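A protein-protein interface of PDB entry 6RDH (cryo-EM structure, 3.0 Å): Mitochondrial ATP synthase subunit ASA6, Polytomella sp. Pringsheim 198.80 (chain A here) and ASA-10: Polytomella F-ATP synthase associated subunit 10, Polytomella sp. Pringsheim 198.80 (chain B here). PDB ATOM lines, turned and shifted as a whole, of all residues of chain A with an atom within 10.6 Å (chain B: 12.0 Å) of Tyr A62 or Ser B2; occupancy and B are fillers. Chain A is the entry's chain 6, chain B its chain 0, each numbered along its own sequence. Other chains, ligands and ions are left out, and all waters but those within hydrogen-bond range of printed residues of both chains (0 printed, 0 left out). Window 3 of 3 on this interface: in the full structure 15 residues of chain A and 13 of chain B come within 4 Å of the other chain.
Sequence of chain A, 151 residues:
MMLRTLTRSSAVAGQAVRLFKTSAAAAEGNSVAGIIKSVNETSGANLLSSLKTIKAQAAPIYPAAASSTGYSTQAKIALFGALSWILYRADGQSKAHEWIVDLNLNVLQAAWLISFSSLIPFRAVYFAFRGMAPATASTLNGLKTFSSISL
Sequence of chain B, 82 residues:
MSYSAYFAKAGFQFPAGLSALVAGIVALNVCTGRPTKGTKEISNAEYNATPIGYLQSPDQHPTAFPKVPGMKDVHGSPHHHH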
ATOM      1  N   GLU A  28      37.303  10.798  -1.658  1.00  0.00           N
ATOM      2  CA  GLU A  28      36.399   9.795  -1.114  1.00  0.00           C
ATOM      3  C   GLU A  28      36.058   8.742  -2.162  1.00  0.00           C
ATOM      4  O   GLU A  28      35.219   8.969  -3.031  1.00  0.00           O
ATOM      5  CB  GLU A  28      35.127  10.458  -0.599  1.00  0.00           C
ATOM      6  CG  GLU A  28      34.171   9.517   0.094  1.00  0.00           C
ATOM      7  CD  GLU A  28      32.769  10.077   0.155  1.00  0.00           C
ATOM      8  OE1 GLU A  28      32.404  10.852  -0.751  1.00  0.00           O
ATOM      9  OE2 GLU A  28      32.032   9.745   1.104  1.00  0.00           O
ATOM     10  N   LYS A  55      30.085  -3.165   7.537  1.00  0.00           N
ATOM     11  CA  LYS A  55      28.741  -2.721   7.198  1.00  0.00           C
ATOM     12  C   LYS A  55      28.523  -1.274   7.609  1.00  0.00           C
ATOM     13  O   LYS A  55      27.901  -0.503   6.874  1.00  0.00           O
ATOM     14  CB  LYS A  55      27.718  -3.628   7.870  1.00  0.00           C
ATOM     15  CG  LYS A  55      26.279  -3.260   7.633  1.00  0.00           C
ATOM     16  CD  LYS A  55      25.791  -3.797   6.316  1.00  0.00           C
ATOM     17  CE  LYS A  55      24.277  -3.840   6.288  1.00  0.00           C
ATOM     18  NZ  LYS A  55      23.756  -4.632   5.140  1.00  0.00           N
ATOM     19  N   ALA A  56      29.047  -0.878   8.767  1.00  0.00           N
ATOM     20  CA  ALA A  56      28.876   0.486   9.240  1.00  0.00           C
ATOM     21  C   ALA A  56      29.903   1.449   8.669  1.00  0.00           C
ATOM     22  O   ALA A  56      29.662   2.655   8.677  1.00  0.00           O
ATOM     23  CB  ALA A  56      28.937   0.522  10.763  1.00  0.00           C
ATOM     24  N   GLN A  57      31.043   0.955   8.190  1.00  0.00           N
ATOM     25  CA  GLN A  57      32.009   1.826   7.535  1.00  0.00           C
ATOM     26  C   GLN A  57      31.552   2.270   6.160  1.00  0.00           C
ATOM     27  O   GLN A  57      32.047   3.279   5.655  1.00  0.00           O
ATOM     28  CB  GLN A  57      33.354   1.128   7.378  1.00  0.00           C
ATOM     29  CG  GLN A  57      34.351   1.395   8.465  1.00  0.00           C
ATOM     30  CD  GLN A  57      35.713   0.841   8.111  1.00  0.00           C
ATOM     31  OE1 GLN A  57      35.959   0.468   6.965  1.00  0.00           O
ATOM     32  NE2 GLN A  57      36.603   0.775   9.092  1.00  0.00           N
ATOM     33  N   ALA A  58      30.650   1.527   5.530  1.00  0.00           N
ATOM     34  CA  ALA A  58      30.200   1.828   4.181  1.00  0.00           C
ATOM     35  C   ALA A  58      28.734   2.216   4.120  1.00  0.00           C
ATOM     36  O   ALA A  58      28.194   2.376   3.025  1.00  0.00           O
ATOM     37  CB  ALA A  58      30.454   0.639   3.268  1.00  0.00           C
ATOM     38  N   ALA A  59      28.072   2.346   5.258  1.00  0.00           N
ATOM     39  CA  ALA A  59      26.746   2.928   5.271  1.00  0.00           C
ATOM     40  C   ALA A  59      26.855   4.424   5.000  1.00  0.00           C
ATOM     41  O   ALA A  59      27.786   5.066   5.488  1.00  0.00           O
ATOM     42  CB  ALA A  59      26.071   2.682   6.614  1.00  0.00           C
ATOM     43  N   PRO A  60      25.936   5.001   4.224  1.00  0.00           N
ATOM     44  CA  PRO A  60      26.077   6.403   3.823  1.00  0.00           C
ATOM     45  C   PRO A  60      25.868   7.355   4.986  1.00  0.00           C
ATOM     46  O   PRO A  60      25.289   7.006   6.012  1.00  0.00           O
ATOM     47  CB  PRO A  60      24.982   6.572   2.773  1.00  0.00           C
ATOM     48  CG  PRO A  60      23.999   5.551   3.107  1.00  0.00           C
ATOM     49  CD  PRO A  60      24.755   4.384   3.603  1.00  0.00           C
ATOM     50  N   ILE A  61      26.371   8.574   4.828  1.00  0.00           N
ATOM     51  CA  ILE A  61      26.281   9.532   5.918  1.00  0.00           C
ATOM     52  C   ILE A  61      24.908  10.181   5.900  1.00  0.00           C
ATOM     53  O   ILE A  61      24.478  10.761   4.900  1.00  0.00           O
ATOM     54  CB  ILE A  61      27.418  10.571   5.864  1.00  0.00           C
ATOM     55  CG1 ILE A  61      27.201  11.621   6.946  1.00  0.00           C
ATOM     56  CG2 ILE A  61      27.582  11.222   4.495  1.00  0.00           C
ATOM     57  CD1 ILE A  61      28.353  12.560   7.146  1.00  0.00           C
ATOM     58  N   TYR A  62      24.187  10.021   6.995  1.00  0.00           N
ATOM     59  CA  TYR A  62      22.957  10.760   7.240  1.00  0.00           C
ATOM     60  C   TYR A  62      23.291  11.699   8.379  1.00  0.00           C
ATOM     61  O   TYR A  62      23.404  11.251   9.533  1.00  0.00           O
ATOM     62  CB  TYR A  62      21.816   9.831   7.618  1.00  0.00           C
ATOM     63  CG  TYR A  62      21.549   8.751   6.617  1.00  0.00           C
ATOM     64  CD1 TYR A  62      21.552   9.019   5.268  1.00  0.00           C
ATOM     65  CD2 TYR A  62      21.276   7.462   7.025  1.00  0.00           C
ATOM     66  CE1 TYR A  62      21.294   8.037   4.355  1.00  0.00           C
ATOM     67  CE2 TYR A  62      21.021   6.475   6.118  1.00  0.00           C
ATOM     68  CZ  TYR A  62      21.031   6.770   4.788  1.00  0.00           C
ATOM     69  OH  TYR A  62      20.775   5.780   3.883  1.00  0.00           O
ATOM     70  N   PRO A  63      23.503  12.984   8.106  1.00  0.00           N
ATOM     71  CA  PRO A  63      23.992  13.889   9.145  1.00  0.00           C
ATOM     72  C   PRO A  63      22.945  14.126  10.215  1.00  0.00           C
ATOM     73  O   PRO A  63      21.753  14.240   9.927  1.00  0.00           O
ATOM     74  CB  PRO A  63      24.303  15.171   8.369  1.00  0.00           C
ATOM     75  CG  PRO A  63      24.426  14.739   6.965  1.00  0.00           C
ATOM     76  CD  PRO A  63      23.436  13.658   6.808  1.00  0.00           C
ATOM     77  N   ALA A  64      23.399  14.151  11.463  1.00  0.00           N
ATOM     78  CA  ALA A  64      22.499  14.243  12.594  1.00  0.00           C
ATOM     79  C   ALA A  64      21.970  15.663  12.744  1.00  0.00           C
ATOM     80  O   ALA A  64      22.481  16.617  12.155  1.00  0.00           O
ATOM     81  CB  ALA A  64      23.200  13.800  13.872  1.00  0.00           C
ATOM     82  N   ALA A  65      20.925  15.789  13.552  1.00  0.00           N
ATOM     83  CA  ALA A  65      20.250  17.063  13.767  1.00  0.00           C
ATOM     84  C   ALA A  65      21.151  17.966  14.591  1.00  0.00           C
ATOM     85  O   ALA A  65      21.280  17.798  15.804  1.00  0.00           O
ATOM     86  CB  ALA A  65      18.910  16.838  14.456  1.00  0.00           C
ATOM     87  N   ALA A  66      21.781  18.932  13.930  1.00  0.00           N
ATOM     88  CA  ALA A  66      22.651  19.867  14.616  1.00  0.00           C
ATOM     89  C   ALA A  66      21.825  20.859  15.435  1.00  0.00           C
ATOM     90  O   ALA A  66      20.598  20.929  15.322  1.00  0.00           O
ATOM     91  CB  ALA A  66      23.541  20.598  13.615  1.00  0.00           C
ATOM     92  N   SER B   2      18.435   9.674   8.385  1.00  0.00           N
ATOM     93  CA  SER B   2      18.085   9.324   7.022  1.00  0.00           C
ATOM     94  C   SER B   2      17.622  10.554   6.279  1.00  0.00           C
ATOM     95  O   SER B   2      16.461  10.650   5.909  1.00  0.00           O
ATOM     96  CB  SER B   2      17.009   8.248   7.009  1.00  0.00           C
ATOM     97  OG  SER B   2      17.581   6.975   7.241  1.00  0.00           O
ATOM     98  N   TYR B   3      18.536  11.520   6.153  1.00  0.00           N
ATOM     99  CA  TYR B   3      18.450  12.737   5.341  1.00  0.00           C
ATOM    100  C   TYR B   3      17.421  13.749   5.813  1.00  0.00           C
ATOM    101  O   TYR B   3      17.364  14.848   5.268  1.00  0.00           O
ATOM    102  CB  TYR B   3      18.152  12.425   3.878  1.00  0.00           C
ATOM    103  CG  TYR B   3      19.306  11.865   3.121  1.00  0.00           C
ATOM    104  CD1 TYR B   3      20.574  12.346   3.314  1.00  0.00           C
ATOM    105  CD2 TYR B   3      19.121  10.845   2.215  1.00  0.00           C
ATOM    106  CE1 TYR B   3      21.625  11.820   2.641  1.00  0.00           C
ATOM    107  CE2 TYR B   3      20.164  10.322   1.529  1.00  0.00           C
ATOM    108  CZ  TYR B   3      21.416  10.811   1.747  1.00  0.00           C
ATOM    109  OH  TYR B   3      22.482  10.292   1.067  1.00  0.00           O
ATOM    110  N   SER B   4      16.620  13.421   6.818  1.00  0.00           N
ATOM    111  CA  SER B   4      15.631  14.370   7.301  1.00  0.00           C
ATOM    112  C   SER B   4      16.268  15.486   8.099  1.00  0.00           C
ATOM    113  O   SER B   4      15.734  16.595   8.142  1.00  0.00           O
ATOM    114  CB  SER B   4      14.598  13.661   8.158  1.00  0.00           C
ATOM    115  OG  SER B   4      13.729  14.602   8.748  1.00  0.00           O
ATOM    116  N   ALA B   5      17.395  15.212   8.730  1.00  0.00           N
ATOM    117  CA  ALA B   5      18.113  16.191   9.520  1.00  0.00           C
ATOM    118  C   ALA B   5      19.138  16.951   8.709  1.00  0.00           C
ATOM    119  O   ALA B   5      19.821  17.817   9.257  1.00  0.00           O
ATOM    120  CB  ALA B   5      18.794  15.501  10.693  1.00  0.00           C
ATOM    121  N   TYR B   6      19.278  16.636   7.430  1.00  0.00           N
ATOM    122  CA  TYR B   6      20.131  17.436   6.569  1.00  0.00           C
ATOM    123  C   TYR B   6      19.376  18.622   6.003  1.00  0.00           C
ATOM    124  O   TYR B   6      19.967  19.682   5.789  1.00  0.00           O
ATOM    125  CB  TYR B   6      20.686  16.570   5.447  1.00  0.00           C
ATOM    126  CG  TYR B   6      21.330  17.332   4.330  1.00  0.00           C
ATOM    127  CD1 TYR B   6      22.472  18.070   4.542  1.00  0.00           C
ATOM    128  CD2 TYR B   6      20.797  17.303   3.062  1.00  0.00           C
ATOM    129  CE1 TYR B   6      23.056  18.763   3.520  1.00  0.00           C
ATOM    130  CE2 TYR B   6      21.373  17.985   2.041  1.00  0.00           C
ATOM    131  CZ  TYR B   6      22.501  18.713   2.270  1.00  0.00           C
ATOM    132  OH  TYR B   6      23.083  19.405   1.240  1.00  0.00           O
ATOM    133  N   PHE B   7      18.075  18.473   5.777  1.00  0.00           N
ATOM    134  CA  PHE B   7      17.286  19.575   5.257  1.00  0.00           C
ATOM    135  C   PHE B   7      16.844  20.532   6.341  1.00  0.00           C
ATOM    136  O   PHE B   7      16.567  21.695   6.043  1.00  0.00           O
ATOM    137  CB  PHE B   7      16.074  19.044   4.512  1.00  0.00           C
ATOM    138  CG  PHE B   7      16.430  18.206   3.349  1.00  0.00           C
ATOM    139  CD1 PHE B   7      17.197  18.720   2.325  1.00  0.00           C
ATOM    140  CD2 PHE B   7      16.015  16.907   3.279  1.00  0.00           C
ATOM    141  CE1 PHE B   7      17.535  17.943   1.267  1.00  0.00           C
ATOM    142  CE2 PHE B   7      16.354  16.133   2.226  1.00  0.00           C
ATOM    143  CZ  PHE B   7      17.108  16.648   1.219  1.00  0.00           C
ATOM    144  N   ALA B   8      16.791  20.079   7.589  1.00  0.00           N
ATOM    145  CA  ALA B   8      16.493  20.982   8.684  1.00  0.00           C
ATOM    146  C   ALA B   8      17.657  21.909   8.994  1.00  0.00           C
ATOM    147  O   ALA B   8      17.463  22.912   9.685  1.00  0.00           O
ATOM    148  CB  ALA B   8      16.109  20.184   9.923  1.00  0.00           C
ATOM    149  N   LYS B   9      18.856  21.596   8.504  1.00  0.00           N
ATOM    150  CA  LYS B   9      20.006  22.459   8.736  1.00  0.00           C
ATOM    151  C   LYS B   9      19.883  23.757   7.957  1.00  0.00           C
ATOM    152  O   LYS B   9      20.115  24.841   8.499  1.00  0.00           O
ATOM    153  CB  LYS B   9      21.294  21.734   8.356  1.00  0.00           C
ATOM    154  CG  LYS B   9      21.659  20.606   9.290  1.00  0.00           C
ATOM    155  CD  LYS B   9      23.004  20.019   8.918  1.00  0.00           C
ATOM    156  CE  LYS B   9      23.340  18.826   9.780  1.00  0.00           C
ATOM    157  NZ  LYS B   9      24.690  18.318   9.468  1.00  0.00           N
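Hydrophobic or aromatic side chains of chain B within 4 Å of the printed part of chain A: Tyr B3 and Ala B5. Printed residues of chain A that touch a printed residue of chain B: Ile A61, Tyr A62, Pro A63, Ala A64 and Ala A65. Among the printed residues, 8 pairs touch across the chains. Among the printed residues, no Asp or Glu carboxylate lies within 4 Å of a Lys or Arg side-chain nitrogen of the other chain.
Gln A57 touches none of the printed residues of chain B. Tyr A62 touches just these residues of chain B: Ser B2 (3.5 Å) and Tyr B3 (3.8 Å). Of the printed residues of chain B, Pro A63 touches Ala B5 and Lys B9. Ala A64 touches just these residues of chain B: Ala B5 (3.8 Å) and Lys B9 (3.4 Å). Of the printed residues of chain B, Ala A65 touches Ala B5. Of the printed residues of chain A, Ser B2 touches Tyr A62. No residue of chain A comes within 4 Å of Ser B4. Printed residues of chain A within 4 Å of Ala B5: Pro A63, Ala A64 and Ala A65. Of the printed residues of chain A, Lys B9 touches Pro A63 (3.4 Å) and Ala A64 (3.4 Å). The nearest residue of chain B that does not touch Tyr A62 is Tyr B6 (6.3 Å). The nearest residue of chain A that does not touch Ser B2 is Pro A63 (5.9 Å).
Ile A61 touches Tyr B3 (O to CE1, 3.8 Å). CB of Tyr A62 touches N of Ser B2, 3.5 Å away. CE2 of Tyr B3 touches CE1 of Tyr A62, at 3.8 Å. Pro A63 touches Ala B5 (O to CB, 3.3 Å). CB of Pro A63 touches NZ of Lys B9, at 3.4 Å. C of Ala A64 touches CB of Ala B5, 3.8 Å away. Lys B9 touches Ala A64 (CE to O, 3.4 Å). N of Ala A65 touches CB of Ala B5 (3.6 Å).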
